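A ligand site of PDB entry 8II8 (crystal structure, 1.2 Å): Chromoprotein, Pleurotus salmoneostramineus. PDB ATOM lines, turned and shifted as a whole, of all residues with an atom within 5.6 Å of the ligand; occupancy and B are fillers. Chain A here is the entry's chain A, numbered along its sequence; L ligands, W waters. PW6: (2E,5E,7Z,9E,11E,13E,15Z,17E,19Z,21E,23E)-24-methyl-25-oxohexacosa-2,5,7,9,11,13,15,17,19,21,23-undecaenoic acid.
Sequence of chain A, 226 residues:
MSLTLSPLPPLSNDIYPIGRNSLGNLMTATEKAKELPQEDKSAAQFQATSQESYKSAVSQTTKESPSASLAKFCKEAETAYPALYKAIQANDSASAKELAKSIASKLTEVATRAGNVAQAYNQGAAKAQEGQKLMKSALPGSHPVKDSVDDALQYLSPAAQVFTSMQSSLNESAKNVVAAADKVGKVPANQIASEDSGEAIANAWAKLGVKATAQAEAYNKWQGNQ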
ATOM      1  N   TYR A  16     -30.813 -37.978 -21.789  1.00  0.00           N
ATOM      2  CA  TYR A  16     -30.839 -36.522 -21.907  1.00  0.00           C
ATOM      3  C   TYR A  16     -29.903 -35.967 -20.848  1.00  0.00           C
ATOM      4  O   TYR A  16     -29.951 -36.382 -19.705  1.00  0.00           O
ATOM      5  CB  TYR A  16     -32.273 -36.064 -21.674  1.00  0.00           C
ATOM      6  CG  TYR A  16     -32.500 -34.593 -21.846  1.00  0.00           C
ATOM      7  CD1 TYR A  16     -32.370 -33.966 -23.046  1.00  0.00           C
ATOM      8  CD2 TYR A  16     -32.848 -33.809 -20.765  1.00  0.00           C
ATOM      9  CE1 TYR A  16     -32.627 -32.610 -23.212  1.00  0.00           C
ATOM     10  CE2 TYR A  16     -33.079 -32.447 -20.900  1.00  0.00           C
ATOM     11  CZ  TYR A  16     -32.952 -31.826 -22.112  1.00  0.00           C
ATOM     12  OH  TYR A  16     -33.151 -30.479 -22.301  1.00  0.00           O
ATOM     13  N   ILE A  18     -29.462 -33.271 -19.105  1.00  0.00           N
ATOM     14  CA  ILE A  18     -29.924 -32.367 -18.060  1.00  0.00           C
ATOM     15  C   ILE A  18     -31.029 -33.063 -17.260  1.00  0.00           C
ATOM     16  O   ILE A  18     -32.111 -33.396 -17.780  1.00  0.00           O
ATOM     17  CB  ILE A  18     -30.407 -31.025 -18.676  1.00  0.00           C
ATOM     18  CG1 ILE A  18     -29.383 -30.412 -19.660  1.00  0.00           C
ATOM     19  CG2 ILE A  18     -30.814 -30.103 -17.526  1.00  0.00           C
ATOM     20  CD1 ILE A  18     -29.630 -30.791 -21.173  1.00  0.00           C
ATOM     21  N   LEU A  23     -27.537 -33.692 -12.224  1.00  0.00           N
ATOM     22  CA  LEU A  23     -27.698 -32.553 -11.332  1.00  0.00           C
ATOM     23  C   LEU A  23     -28.238 -32.997  -9.979  1.00  0.00           C
ATOM     24  O   LEU A  23     -28.481 -32.166  -9.107  1.00  0.00           O
ATOM     25  CB  LEU A  23     -28.622 -31.505 -11.956  1.00  0.00           C
ATOM     26  CG  LEU A  23     -28.152 -30.932 -13.288  1.00  0.00           C
ATOM     27  CD1 LEU A  23     -29.268 -30.177 -13.988  1.00  0.00           C
ATOM     28  CD2 LEU A  23     -26.920 -30.079 -13.105  1.00  0.00           C
ATOM     29  N   LEU A  26     -26.478 -31.706  -6.728  1.00  0.00           N
ATOM     30  CA  LEU A  26     -26.757 -30.293  -6.502  1.00  0.00           C
ATOM     31  C   LEU A  26     -28.203 -30.092  -6.059  1.00  0.00           C
ATOM     32  O   LEU A  26     -28.497 -29.273  -5.204  1.00  0.00           O
ATOM     33  CB  LEU A  26     -26.435 -29.481  -7.751  1.00  0.00           C
ATOM     34  CG  LEU A  26     -26.642 -27.971  -7.680  1.00  0.00           C
ATOM     35  CD1 LEU A  26     -25.786 -27.330  -6.604  1.00  0.00           C
ATOM     36  CD2 LEU A  26     -26.322 -27.355  -9.019  1.00  0.00           C
ATOM     37  N   MET A  27     -29.151 -30.878  -6.609  1.00  0.00           N
ATOM     38  CA  MET A  27     -30.536 -30.791  -6.207  1.00  0.00           C
ATOM     39  C   MET A  27     -30.682 -31.163  -4.737  1.00  0.00           C
ATOM     40  O   MET A  27     -31.378 -30.516  -3.971  1.00  0.00           O
ATOM     41  CB  MET A  27     -31.390 -31.689  -7.107  1.00  0.00           C
ATOM     42  CG  MET A  27     -31.518 -31.087  -8.513  1.00  0.00           C
ATOM     43  SD  MET A  27     -32.214 -32.245  -9.731  1.00  0.00           S
ATOM     44  CE  MET A  27     -33.912 -32.249  -9.180  1.00  0.00           C
ATOM     45  N   THR A  30     -29.490 -28.474  -2.537  1.00  0.00           N
ATOM     46  CA  THR A  30     -30.409 -27.365  -2.520  1.00  0.00           C
ATOM     47  C   THR A  30     -31.602 -27.611  -1.588  1.00  0.00           C
ATOM     48  O   THR A  30     -32.028 -26.739  -0.824  1.00  0.00           O
ATOM     49  CB  THR A  30     -30.885 -27.090  -3.952  1.00  0.00           C
ATOM     50  OG1 THR A  30     -29.747 -26.798  -4.784  1.00  0.00           O
ATOM     51  CG2 THR A  30     -31.894 -25.961  -3.965  1.00  0.00           C
ATOM     52  N   PHE A  46     -25.476 -15.616   8.168  1.00  0.00           N
ATOM     53  CA  PHE A  46     -24.790 -16.355   7.131  1.00  0.00           C
ATOM     54  C   PHE A  46     -25.695 -17.376   6.469  1.00  0.00           C
ATOM     55  O   PHE A  46     -25.600 -17.597   5.262  1.00  0.00           O
ATOM     56  CB  PHE A  46     -23.603 -17.117   7.727  1.00  0.00           C
ATOM     57  CG  PHE A  46     -22.496 -16.273   8.255  1.00  0.00           C
ATOM     58  CD1 PHE A  46     -21.848 -15.424   7.413  1.00  0.00           C
ATOM     59  CD2 PHE A  46     -22.067 -16.388   9.568  1.00  0.00           C
ATOM     60  CE1 PHE A  46     -20.743 -14.697   7.865  1.00  0.00           C
ATOM     61  CE2 PHE A  46     -21.005 -15.636  10.041  1.00  0.00           C
ATOM     62  CZ  PHE A  46     -20.337 -14.794   9.174  1.00  0.00           C
ATOM     63  N   THR A  49     -28.112 -15.664   4.056  1.00  0.00           N
ATOM     64  CA  THR A  49     -27.400 -15.294   2.857  1.00  0.00           C
ATOM     65  C   THR A  49     -27.174 -16.519   1.981  1.00  0.00           C
ATOM     66  O   THR A  49     -27.313 -16.461   0.756  1.00  0.00           O
ATOM     67  CB  THR A  49     -26.112 -14.539   3.195  1.00  0.00           C
ATOM     68  OG1 THR A  49     -26.483 -13.368   3.918  1.00  0.00           O
ATOM     69  CG2 THR A  49     -25.292 -14.204   1.960  1.00  0.00           C
ATOM     70  N   SER A  50     -26.753 -17.633   2.607  1.00  0.00           N
ATOM     71  CA  SER A  50     -26.513 -18.867   1.872  1.00  0.00           C
ATOM     72  C   SER A  50     -27.806 -19.344   1.203  1.00  0.00           C
ATOM     73  O   SER A  50     -27.823 -19.758   0.043  1.00  0.00           O
ATOM     74  CB  SER A  50     -25.996 -19.945   2.792  1.00  0.00           C
ATOM     75  OG  SER A  50     -24.752 -19.609   3.396  1.00  0.00           O
ATOM     76  N   SER A  53     -28.691 -17.299  -1.720  1.00  0.00           N
ATOM     77  CA  SER A  53     -27.852 -17.581  -2.858  1.00  0.00           C
ATOM     78  C   SER A  53     -28.355 -18.812  -3.614  1.00  0.00           C
ATOM     79  O   SER A  53     -28.440 -18.810  -4.841  1.00  0.00           O
ATOM     80  CB  SER A  53     -26.386 -17.755  -2.454  1.00  0.00           C
ATOM     81  OG  SER A  53     -25.885 -16.622  -1.758  1.00  0.00           O
ATOM     82  N   TYR A  54     -28.689 -19.879  -2.902  1.00  0.00           N
ATOM     83  CA  TYR A  54     -29.290 -21.058  -3.506  1.00  0.00           C
ATOM     84  C   TYR A  54     -30.585 -20.664  -4.218  1.00  0.00           C
ATOM     85  O   TYR A  54     -30.873 -21.092  -5.331  1.00  0.00           O
ATOM     86  CB  TYR A  54     -29.569 -22.139  -2.464  1.00  0.00           C
ATOM     87  CG  TYR A  54     -28.442 -23.117  -2.217  1.00  0.00           C
ATOM     88  CD1 TYR A  54     -28.334 -24.260  -2.966  1.00  0.00           C
ATOM     89  CD2 TYR A  54     -27.519 -22.944  -1.183  1.00  0.00           C
ATOM     90  CE1 TYR A  54     -27.366 -25.215  -2.746  1.00  0.00           C
ATOM     91  CE2 TYR A  54     -26.555 -23.911  -0.942  1.00  0.00           C
ATOM     92  CZ  TYR A  54     -26.461 -25.051  -1.721  1.00  0.00           C
ATOM     93  OH  TYR A  54     -25.527 -26.054  -1.506  1.00  0.00           O
ATOM     94  N   ALA A  57     -30.235 -18.682  -7.518  1.00  0.00           N
ATOM     95  CA  ALA A  57     -29.784 -19.513  -8.613  1.00  0.00           C
ATOM     96  C   ALA A  57     -30.910 -20.385  -9.165  1.00  0.00           C
ATOM     97  O   ALA A  57     -31.000 -20.553 -10.383  1.00  0.00           O
ATOM     98  CB  ALA A  57     -28.616 -20.355  -8.197  1.00  0.00           C
ATOM     99  N   VAL A  58     -31.706 -20.973  -8.287  1.00  0.00           N
ATOM    100  CA  VAL A  58     -32.859 -21.765  -8.743  1.00  0.00           C
ATOM    101  C   VAL A  58     -33.867 -20.848  -9.437  1.00  0.00           C
ATOM    102  O   VAL A  58     -34.378 -21.191 -10.498  1.00  0.00           O
ATOM    103  CB  VAL A  58     -33.478 -22.537  -7.573  1.00  0.00           C
ATOM    104  CG1 VAL A  58     -34.784 -23.237  -7.984  1.00  0.00           C
ATOM    105  CG2 VAL A  58     -32.514 -23.580  -6.982  1.00  0.00           C
ATOM    106  N   THR A  61     -32.645 -20.171 -12.804  1.00  0.00           N
ATOM    107  CA  THR A  61     -32.850 -21.375 -13.610  1.00  0.00           C
ATOM    108  C   THR A  61     -34.272 -21.429 -14.160  1.00  0.00           C
ATOM    109  O   THR A  61     -34.490 -21.735 -15.328  1.00  0.00           O
ATOM    110  CB  THR A  61     -32.491 -22.617 -12.811  1.00  0.00           C
ATOM    111  OG1 THR A  61     -31.147 -22.505 -12.326  1.00  0.00           O
ATOM    112  CG2 THR A  61     -32.587 -23.873 -13.639  1.00  0.00           C
ATOM    113  N   SER A  65     -35.405 -21.629 -17.962  1.00  0.00           N
ATOM    114  CA  SER A  65     -36.031 -22.887 -18.312  1.00  0.00           C
ATOM    115  C   SER A  65     -35.549 -23.392 -19.657  1.00  0.00           C
ATOM    116  O   SER A  65     -36.316 -23.536 -20.630  1.00  0.00           O
ATOM    117  CB  SER A  65     -37.540 -22.808 -18.218  1.00  0.00           C
ATOM    118  OG  SER A  65     -37.930 -22.711 -16.821  1.00  0.00           O
ATOM    119  N   PRO A  66     -34.267 -23.758 -19.770  1.00  0.00           N
ATOM    120  CA  PRO A  66     -33.729 -24.140 -21.059  1.00  0.00           C
ATOM    121  C   PRO A  66     -34.382 -25.393 -21.663  1.00  0.00           C
ATOM    122  O   PRO A  66     -34.573 -25.473 -22.853  1.00  0.00           O
ATOM    123  CB  PRO A  66     -32.238 -24.341 -20.812  1.00  0.00           C
ATOM    124  CG  PRO A  66     -32.015 -23.894 -19.494  1.00  0.00           C
ATOM    125  CD  PRO A  66     -33.231 -23.665 -18.716  1.00  0.00           C
ATOM    126  N   SER A  67     -34.688 -26.417 -20.841  1.00  0.00           N
ATOM    127  CA  SER A  67     -35.307 -27.627 -21.376  1.00  0.00           C
ATOM    128  C   SER A  67     -36.696 -27.343 -21.955  1.00  0.00           C
ATOM    129  O   SER A  67     -37.051 -27.828 -23.017  1.00  0.00           O
ATOM    130  CB  SER A  67     -35.367 -28.747 -20.365  1.00  0.00           C
ATOM    131  OG  SER A  67     -34.076 -29.208 -20.059  1.00  0.00           O
ATOM    132  N   ALA A  68     -37.500 -26.520 -21.250  1.00  0.00           N
ATOM    133  CA  ALA A  68     -38.815 -26.128 -21.763  1.00  0.00           C
ATOM    134  C   ALA A  68     -38.642 -25.383 -23.097  1.00  0.00           C
ATOM    135  O   ALA A  68     -39.389 -25.597 -24.029  1.00  0.00           O
ATOM    136  CB  ALA A  68     -39.562 -25.273 -20.779  1.00  0.00           C
ATOM    137  N   ALA A 120     -25.212 -18.181 -13.940  1.00  0.00           N
ATOM    138  CA  ALA A 120     -25.750 -18.091 -12.599  1.00  0.00           C
ATOM    139  C   ALA A 120     -25.023 -19.061 -11.654  1.00  0.00           C
ATOM    140  O   ALA A 120     -24.738 -18.719 -10.504  1.00  0.00           O
ATOM    141  CB  ALA A 120     -27.229 -18.401 -12.582  1.00  0.00           C
ATOM    142  N   TYR A 121     -24.715 -20.251 -12.124  1.00  0.00           N
ATOM    143  CA  TYR A 121     -24.071 -21.232 -11.268  1.00  0.00           C
ATOM    144  C   TYR A 121     -22.616 -20.863 -10.987  1.00  0.00           C
ATOM    145  O   TYR A 121     -22.138 -20.981  -9.860  1.00  0.00           O
ATOM    146  CB  TYR A 121     -24.212 -22.637 -11.832  1.00  0.00           C
ATOM    147  CG  TYR A 121     -25.632 -23.180 -11.884  1.00  0.00           C
ATOM    148  CD1 TYR A 121     -26.716 -22.499 -11.403  1.00  0.00           C
ATOM    149  CD2 TYR A 121     -25.860 -24.418 -12.439  1.00  0.00           C
ATOM    150  CE1 TYR A 121     -28.010 -22.989 -11.515  1.00  0.00           C
ATOM    151  CE2 TYR A 121     -27.141 -24.932 -12.567  1.00  0.00           C
ATOM    152  CZ  TYR A 121     -28.217 -24.189 -12.144  1.00  0.00           C
ATOM    153  OH  TYR A 121     -29.488 -24.674 -12.349  1.00  0.00           O
ATOM    154  N   GLY A 124     -22.656 -18.110  -8.605  1.00  0.00           N
ATOM    155  CA  GLY A 124     -23.000 -18.671  -7.316  1.00  0.00           C
ATOM    156  C   GLY A 124     -21.786 -19.292  -6.627  1.00  0.00           C
ATOM    157  O   GLY A 124     -21.648 -19.176  -5.404  1.00  0.00           O
ATOM    158  N   ALA A 125     -20.886 -19.883  -7.407  1.00  0.00           N
ATOM    159  CA  ALA A 125     -19.686 -20.494  -6.829  1.00  0.00           C
ATOM    160  C   ALA A 125     -18.818 -19.432  -6.185  1.00  0.00           C
ATOM    161  O   ALA A 125     -18.234 -19.663  -5.109  1.00  0.00           O
ATOM    162  CB  ALA A 125     -18.924 -21.272  -7.863  1.00  0.00           C
ATOM    163  N   LYS A 127     -19.905 -16.666  -4.767  1.00  0.00           N
ATOM    164  CA  LYS A 127     -20.536 -16.383  -3.489  1.00  0.00           C
ATOM    165  C   LYS A 127     -20.195 -17.434  -2.432  1.00  0.00           C
ATOM    166  O   LYS A 127     -19.878 -17.107  -1.290  1.00  0.00           O
ATOM    167  CB  LYS A 127     -22.066 -16.311  -3.621  1.00  0.00           C
ATOM    168  CG  LYS A 127     -22.534 -15.242  -4.569  1.00  0.00           C
ATOM    169  CD  LYS A 127     -24.044 -15.329  -4.724  1.00  0.00           C
ATOM    170  CE  LYS A 127     -24.673 -14.346  -5.662  1.00  0.00           C
ATOM    171  NZ  LYS A 127     -26.119 -14.646  -5.671  1.00  0.00           N
ATOM    172  N   ALA A 128     -20.247 -18.695  -2.823  1.00  0.00           N
ATOM    173  CA  ALA A 128     -19.928 -19.774  -1.914  1.00  0.00           C
ATOM    174  C   ALA A 128     -18.467 -19.688  -1.462  1.00  0.00           C
ATOM    175  O   ALA A 128     -18.173 -20.007  -0.312  1.00  0.00           O
ATOM    176  CB  ALA A 128     -20.241 -21.107  -2.538  1.00  0.00           C
ATOM    177  N   GLU A 130     -16.763 -16.983  -0.938  1.00  0.00           N
ATOM    178  CA  GLU A 130     -16.742 -15.950   0.097  1.00  0.00           C
ATOM    179  C   GLU A 130     -17.322 -16.512   1.390  1.00  0.00           C
ATOM    180  O   GLU A 130     -16.791 -16.295   2.477  1.00  0.00           O
ATOM    181  CB  GLU A 130     -17.487 -14.702  -0.386  1.00  0.00           C
ATOM    182  CG  GLU A 130     -17.481 -13.507   0.538  1.00  0.00           C
ATOM    183  CD  GLU A 130     -18.219 -12.258   0.014  1.00  0.00           C
ATOM    184  OE1 GLU A 130     -18.596 -12.230  -1.171  1.00  0.00           O
ATOM    185  OE2 GLU A 130     -18.389 -11.315   0.811  1.00  0.00           O
ATOM    186  N   GLY A 131     -18.495 -17.157   1.273  1.00  0.00           N
ATOM    187  CA  GLY A 131     -19.147 -17.702   2.448  1.00  0.00           C
ATOM    188  C   GLY A 131     -18.274 -18.716   3.199  1.00  0.00           C
ATOM    189  O   GLY A 131     -18.245 -18.761   4.415  1.00  0.00           O
ATOM    190  N   LEU A 134     -15.739 -16.817   5.281  1.00  0.00           N
ATOM    191  CA  LEU A 134     -16.360 -16.112   6.397  1.00  0.00           C
ATOM    192  C   LEU A 134     -16.654 -17.100   7.521  1.00  0.00           C
ATOM    193  O   LEU A 134     -16.427 -16.830   8.695  1.00  0.00           O
ATOM    194  CB  LEU A 134     -17.685 -15.496   5.925  1.00  0.00           C
ATOM    195  CG  LEU A 134     -17.587 -14.190   5.133  1.00  0.00           C
ATOM    196  CD1 LEU A 134     -18.889 -13.987   4.385  1.00  0.00           C
ATOM    197  CD2 LEU A 134     -17.295 -13.002   6.023  1.00  0.00           C
ATOM    198  N   MET A 135     -17.277 -18.230   7.147  1.00  0.00           N
ATOM    199  CA  MET A 135     -17.796 -19.145   8.149  1.00  0.00           C
ATOM    200  C   MET A 135     -16.711 -19.997   8.794  1.00  0.00           C
ATOM    201  O   MET A 135     -16.847 -20.406   9.951  1.00  0.00           O
ATOM    202  CB  MET A 135     -18.847 -20.038   7.539  1.00  0.00           C
ATOM    203  CG  MET A 135     -20.100 -19.258   7.148  1.00  0.00           C
ATOM    204  SD  MET A 135     -21.451 -20.301   6.623  1.00  0.00           S
ATOM    205  CE  MET A 135     -20.570 -21.355   5.526  1.00  0.00           C
ATOM    206  N   SER A 148     -23.448 -27.058   3.609  1.00  0.00           N
ATOM    207  CA  SER A 148     -24.182 -26.584   2.459  1.00  0.00           C
ATOM    208  C   SER A 148     -23.333 -25.721   1.513  1.00  0.00           C
ATOM    209  O   SER A 148     -23.481 -25.747   0.300  1.00  0.00           O
ATOM    210  CB  SER A 148     -25.427 -25.847   2.884  1.00  0.00           C
ATOM    211  OG  SER A 148     -26.387 -26.760   3.445  1.00  0.00           O
ATOM    212  N   VAL A 149     -22.488 -24.870   2.093  1.00  0.00           N
ATOM    213  CA  VAL A 149     -21.534 -24.115   1.319  1.00  0.00           C
ATOM    214  C   VAL A 149     -20.537 -25.046   0.616  1.00  0.00           C
ATOM    215  O   VAL A 149     -20.225 -24.866  -0.563  1.00  0.00           O
ATOM    216  CB  VAL A 149     -20.863 -23.042   2.172  1.00  0.00           C
ATOM    217  CG1 VAL A 149     -19.693 -22.399   1.437  1.00  0.00           C
ATOM    218  CG2 VAL A 149     -21.869 -22.026   2.633  1.00  0.00           C
ATOM    219  N   ALA A 152     -22.154 -26.643  -2.379  1.00  0.00           N
ATOM    220  CA  ALA A 152     -22.213 -25.724  -3.510  1.00  0.00           C
ATOM    221  C   ALA A 152     -20.872 -25.694  -4.240  1.00  0.00           C
ATOM    222  O   ALA A 152     -20.807 -25.754  -5.477  1.00  0.00           O
ATOM    223  CB  ALA A 152     -22.625 -24.354  -3.041  1.00  0.00           C
ATOM    224  N   LEU A 156     -21.287 -26.989  -8.067  1.00  0.00           N
ATOM    225  CA  LEU A 156     -21.700 -25.938  -8.987  1.00  0.00           C
ATOM    226  C   LEU A 156     -20.946 -25.961 -10.310  1.00  0.00           C
ATOM    227  O   LEU A 156     -21.559 -25.804 -11.366  1.00  0.00           O
ATOM    228  CB  LEU A 156     -21.617 -24.570  -8.351  1.00  0.00           C
ATOM    229  CG  LEU A 156     -22.769 -24.223  -7.447  1.00  0.00           C
ATOM    230  CD1 LEU A 156     -22.486 -22.994  -6.626  1.00  0.00           C
ATOM    231  CD2 LEU A 156     -24.084 -24.069  -8.258  1.00  0.00           C
ATOM    232  N   PHE A 163     -24.751 -27.137 -18.546  1.00  0.00           N
ATOM    233  CA  PHE A 163     -25.411 -26.087 -19.273  1.00  0.00           C
ATOM    234  C   PHE A 163     -24.543 -25.459 -20.351  1.00  0.00           C
ATOM    235  O   PHE A 163     -25.035 -25.167 -21.446  1.00  0.00           O
ATOM    236  CB  PHE A 163     -26.056 -25.083 -18.337  1.00  0.00           C
ATOM    237  CG  PHE A 163     -27.236 -25.674 -17.622  1.00  0.00           C
ATOM    238  CD1 PHE A 163     -28.451 -25.759 -18.266  1.00  0.00           C
ATOM    239  CD2 PHE A 163     -27.119 -26.255 -16.377  1.00  0.00           C
ATOM    240  CE1 PHE A 163     -29.536 -26.372 -17.667  1.00  0.00           C
ATOM    241  CE2 PHE A 163     -28.206 -26.855 -15.776  1.00  0.00           C
ATOM    242  CZ  PHE A 163     -29.423 -26.925 -16.418  1.00  0.00           C
ATOM    243  N   GLN A 215     -38.099 -33.664 -18.939  1.00  0.00           N
ATOM    244  CA  GLN A 215     -37.240 -32.970 -17.994  1.00  0.00           C
ATOM    245  C   GLN A 215     -37.846 -31.626 -17.587  1.00  0.00           C
ATOM    246  O   GLN A 215     -37.786 -31.220 -16.432  1.00  0.00           O
ATOM    247  CB  GLN A 215     -35.829 -32.769 -18.559  1.00  0.00           C
ATOM    248  CG  GLN A 215     -34.984 -31.769 -17.792  1.00  0.00           C
ATOM    249  CD  GLN A 215     -34.714 -32.009 -16.329  1.00  0.00           C
ATOM    250  OE1 GLN A 215     -34.196 -31.086 -15.665  1.00  0.00           O
ATOM    251  NE2 GLN A 215     -34.999 -33.194 -15.848  1.00  0.00           N
ATOM    252  N   ALA A 216     -38.410 -30.882 -18.554  1.00  0.00           N
ATOM    253  CA  ALA A 216     -38.998 -29.603 -18.217  1.00  0.00           C
ATOM    254  C   ALA A 216     -40.075 -29.773 -17.159  1.00  0.00           C
ATOM    255  O   ALA A 216     -40.187 -28.997 -16.226  1.00  0.00           O
ATOM    256  CB  ALA A 216     -39.520 -28.931 -19.472  1.00  0.00           C
ATOM    257  N   TYR A 219     -38.502 -30.782 -13.735  1.00  0.00           N
ATOM    258  CA  TYR A 219     -37.882 -29.633 -13.106  1.00  0.00           C
ATOM    259  C   TYR A 219     -38.938 -28.670 -12.552  1.00  0.00           C
ATOM    260  O   TYR A 219     -38.793 -28.101 -11.456  1.00  0.00           O
ATOM    261  CB  TYR A 219     -36.958 -28.925 -14.095  1.00  0.00           C
ATOM    262  CG  TYR A 219     -36.412 -27.633 -13.472  1.00  0.00           C
ATOM    263  CD1 TYR A 219     -35.460 -27.659 -12.486  1.00  0.00           C
ATOM    264  CD2 TYR A 219     -36.943 -26.391 -13.821  1.00  0.00           C
ATOM    265  CE1 TYR A 219     -35.054 -26.495 -11.847  1.00  0.00           C
ATOM    266  CE2 TYR A 219     -36.562 -25.210 -13.216  1.00  0.00           C
ATOM    267  CZ  TYR A 219     -35.606 -25.283 -12.203  1.00  0.00           C
ATOM    268  OH  TYR A 219     -35.187 -24.186 -11.500  1.00  0.00           O
ATOM    269  N   TRP A 222     -40.055 -29.755  -9.291  1.00  0.00           N
ATOM    270  CA  TRP A 222     -39.025 -29.660  -8.260  1.00  0.00           C
ATOM    271  C   TRP A 222     -38.848 -28.216  -7.805  1.00  0.00           C
ATOM    272  O   TRP A 222     -38.788 -27.949  -6.599  1.00  0.00           O
ATOM    273  CB  TRP A 222     -37.728 -30.238  -8.800  1.00  0.00           C
ATOM    274  CG  TRP A 222     -36.621 -30.215  -7.784  1.00  0.00           C
ATOM    275  CD1 TRP A 222     -36.416 -31.105  -6.769  1.00  0.00           C
ATOM    276  CD2 TRP A 222     -35.583 -29.233  -7.682  1.00  0.00           C
ATOM    277  NE1 TRP A 222     -35.309 -30.737  -6.060  1.00  0.00           N
ATOM    278  CE2 TRP A 222     -34.759 -29.609  -6.597  1.00  0.00           C
ATOM    279  CE3 TRP A 222     -35.230 -28.096  -8.403  1.00  0.00           C
ATOM    280  CZ2 TRP A 222     -33.659 -28.873  -6.201  1.00  0.00           C
ATOM    281  CZ3 TRP A 222     -34.117 -27.381  -8.041  1.00  0.00           C
ATOM    282  CH2 TRP A 222     -33.355 -27.762  -6.942  1.00  0.00           C
HETATM  283  C4  PW6 L   1     -22.474 -16.233   3.282  1.00  0.00           C
HETATM  284  C14 PW6 L   1     -26.540 -22.471  -5.819  1.00  0.00           C
HETATM  285  C5  PW6 L   1     -22.356 -16.799   0.895  1.00  0.00           C
HETATM  286  C6  PW6 L   1     -22.862 -18.100   0.937  1.00  0.00           C
HETATM  287  C11 PW6 L   1     -24.900 -21.204  -3.561  1.00  0.00           C
HETATM  288  C7  PW6 L   1     -23.206 -18.825  -0.198  1.00  0.00           C
HETATM  289  C8  PW6 L   1     -23.720 -20.107  -0.147  1.00  0.00           C
HETATM  290  C9  PW6 L   1     -24.161 -20.872  -1.225  1.00  0.00           C
HETATM  291  C10 PW6 L   1     -24.215 -20.514  -2.543  1.00  0.00           C
HETATM  292  C12 PW6 L   1     -25.058 -20.745  -4.848  1.00  0.00           C
HETATM  293  C13 PW6 L   1     -25.730 -21.346  -5.866  1.00  0.00           C
HETATM  294  C3  PW6 L   1     -22.149 -15.893   1.910  1.00  0.00           C
HETATM  295  C1  PW6 L   1     -21.387 -14.184   0.217  1.00  0.00           C
HETATM  296  C2  PW6 L   1     -21.710 -14.558   1.618  1.00  0.00           C
HETATM  297  O1  PW6 L   1     -21.634 -13.690   2.525  1.00  0.00           O
HETATM  298  C15 PW6 L   1     -27.175 -23.054  -6.867  1.00  0.00           C
HETATM  299  C16 PW6 L   1     -28.017 -24.198  -6.907  1.00  0.00           C
HETATM  300  C17 PW6 L   1     -28.610 -24.688  -8.024  1.00  0.00           C
HETATM  301  C18 PW6 L   1     -29.392 -25.832  -8.090  1.00  0.00           C
HETATM  302  C19 PW6 L   1     -29.899 -26.414  -9.232  1.00  0.00           C
HETATM  303  C20 PW6 L   1     -30.581 -27.613  -9.309  1.00  0.00           C
HETATM  304  C21 PW6 L   1     -31.111 -28.174 -10.424  1.00  0.00           C
HETATM  305  C22 PW6 L   1     -31.204 -27.608 -11.729  1.00  0.00           C
HETATM  306  C23 PW6 L   1     -31.924 -28.057 -12.739  1.00  0.00           C
HETATM  307  C24 PW6 L   1     -32.096 -27.383 -13.980  1.00  0.00           C
HETATM  308  C25 PW6 L   1     -33.074 -27.643 -14.898  1.00  0.00           C
HETATM  309  C26 PW6 L   1     -33.445 -26.810 -15.944  1.00  0.00           C
HETATM  310  C27 PW6 L   1     -33.902 -27.371 -17.243  1.00  0.00           C
HETATM  311  O2  PW6 L   1     -34.376 -26.538 -18.054  1.00  0.00           O
HETATM  312  O3  PW6 L   1     -33.816 -28.579 -17.441  1.00  0.00           O
HETATM  313  O   HOH W   1     -37.058 -26.116 -18.440  1.00  0.00           O
HETATM  314  O   HOH W   2     -20.963 -11.137   2.261  1.00  0.00           O
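The side-chain hydroxyl (OG1) of Thr 30 lies within hydrogen-bond range of the backbone carbonyl oxygen (O) of Leu 26 (2.8 Å). The side-chain hydroxyl (OG) of Ser 50 is in hydrogen-bond range of the backbone carbonyl oxygen (O) of Phe 46 (2.9 Å). The side-chain amide nitrogen (NE2) of Gln 215 lies close to the backbone carbonyl oxygen (O) of Ile 18, 3.5 Å away. The side-chain hydroxyl (OH) of Tyr 121 sits at hydrogen-bond distance from the side-chain hydroxyl (OG1) of Thr 61 (2.7 Å). The side-chain hydroxyl of Tyr 16 lies within hydrogen-bond range of the side-chain hydroxyl of Ser 67 (2.7 Å). The backbone carbonyl oxygen of Ala 57 lies within hydrogen-bond range of the side-chain hydroxyl of Thr 61 (2.8 Å). The side-chain hydroxyl of Tyr 219 is in hydrogen-bond range of the backbone carbonyl oxygen of Val 58. The side-chain hydroxyl of Ser 53 is in hydrogen-bond range of the backbone carbonyl oxygen of Thr 49.
O2 of the ligand sits close to N of Pro 66 (3.3 Å). CG2 of Ile 18 touches O3 of the ligand, at 3.4 Å. Leu 23 touches the ligand (CD1 to C23, 3.6 Å). CG of Leu 26 touches C18 of the ligand, 3.5 Å away. CG of Met 27 touches C21 of the ligand (3.5 Å). OG1 of Thr 30 touches C18 of the ligand, at 3.5 Å. Phe 46 touches the ligand. Thr 49 touches the ligand. Ser 50 touches the ligand (OG to C6, 3.4 Å). Ser 53 touches the ligand (CB to C10, 3.5 Å). Tyr 54 touches the ligand. Ala 57 touches the ligand. Thr 61 touches the ligand (CG2 to C24, 3.6 Å). Ser 65 touches the ligand (C to O2, 3.7 Å). Tyr 121 touches the ligand. Gly 124 touches the ligand (O to C12, 3.8 Å). Lys 127 touches the ligand (O to C5, 3.3 Å). CA of Ala 128 touches C7 of the ligand, 3.8 Å away. Glu 130 touches the ligand (OE1 to C1, 3.7 Å). Gly 131 touches the ligand. CD1 of Leu 134 touches O1 of the ligand, at 3.3 Å. Val 149 touches the ligand (CG2 to C8, 3.9 Å). Ala 152 touches the ligand (CB to C11, 3.9 Å). Leu 156 touches the ligand (CD2 to C15, 3.5 Å). Phe 163 touches the ligand (CZ to C24, 3.6 Å). Tyr 219 touches the ligand (CD1 to C25, 3.4 Å). CH2 of Trp 222 touches C20 of the ligand (3.6 Å). Hydrophobic or aromatic side chains that line the ligand: Ile 18, Leu 23, Leu 26, Met 27, Tyr 54, Ala 57, Pro 66, Tyr 121, Leu 134, Val 149, Ala 152, Leu 156, Phe 163, Tyr 219 and Trp 222. Within 4 Å of the ligand: Ile 18, Leu 23, Leu 26, Met 27, Thr 30, Phe 46, Thr 49, Ser 50, Ser 53, Tyr 54, Ala 57, Thr 61, Ser 65, Pro 66, Ser 67, Tyr 121, Gly 124, Lys 127, Ala 128, Glu 130, Gly 131, Leu 134, Val 149, Ala 152, Leu 156, Phe 163, Gln 215, Tyr 219 and Trp 222.
Water W2 bridges O1 of the ligand and OE2 of Glu 130. Water W1 lies within hydrogen-bond range of O2 of the ligand (2.7 Å), N of Ala 68 (2.9 Å), N of Ser 67 (3.4 Å) and O of Ser 65 (3.5 Å).
An oxygen (O2) of the ligand is in hydrogen-bond range of the backbone NH (N) of Ser 67. OE1 of Gln 215 sits close to O3 of the ligand (3.1 Å). The side-chain hydroxyl (OG) of Ser 67 is in hydrogen-bond range of an oxygen (O3) of the ligand.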
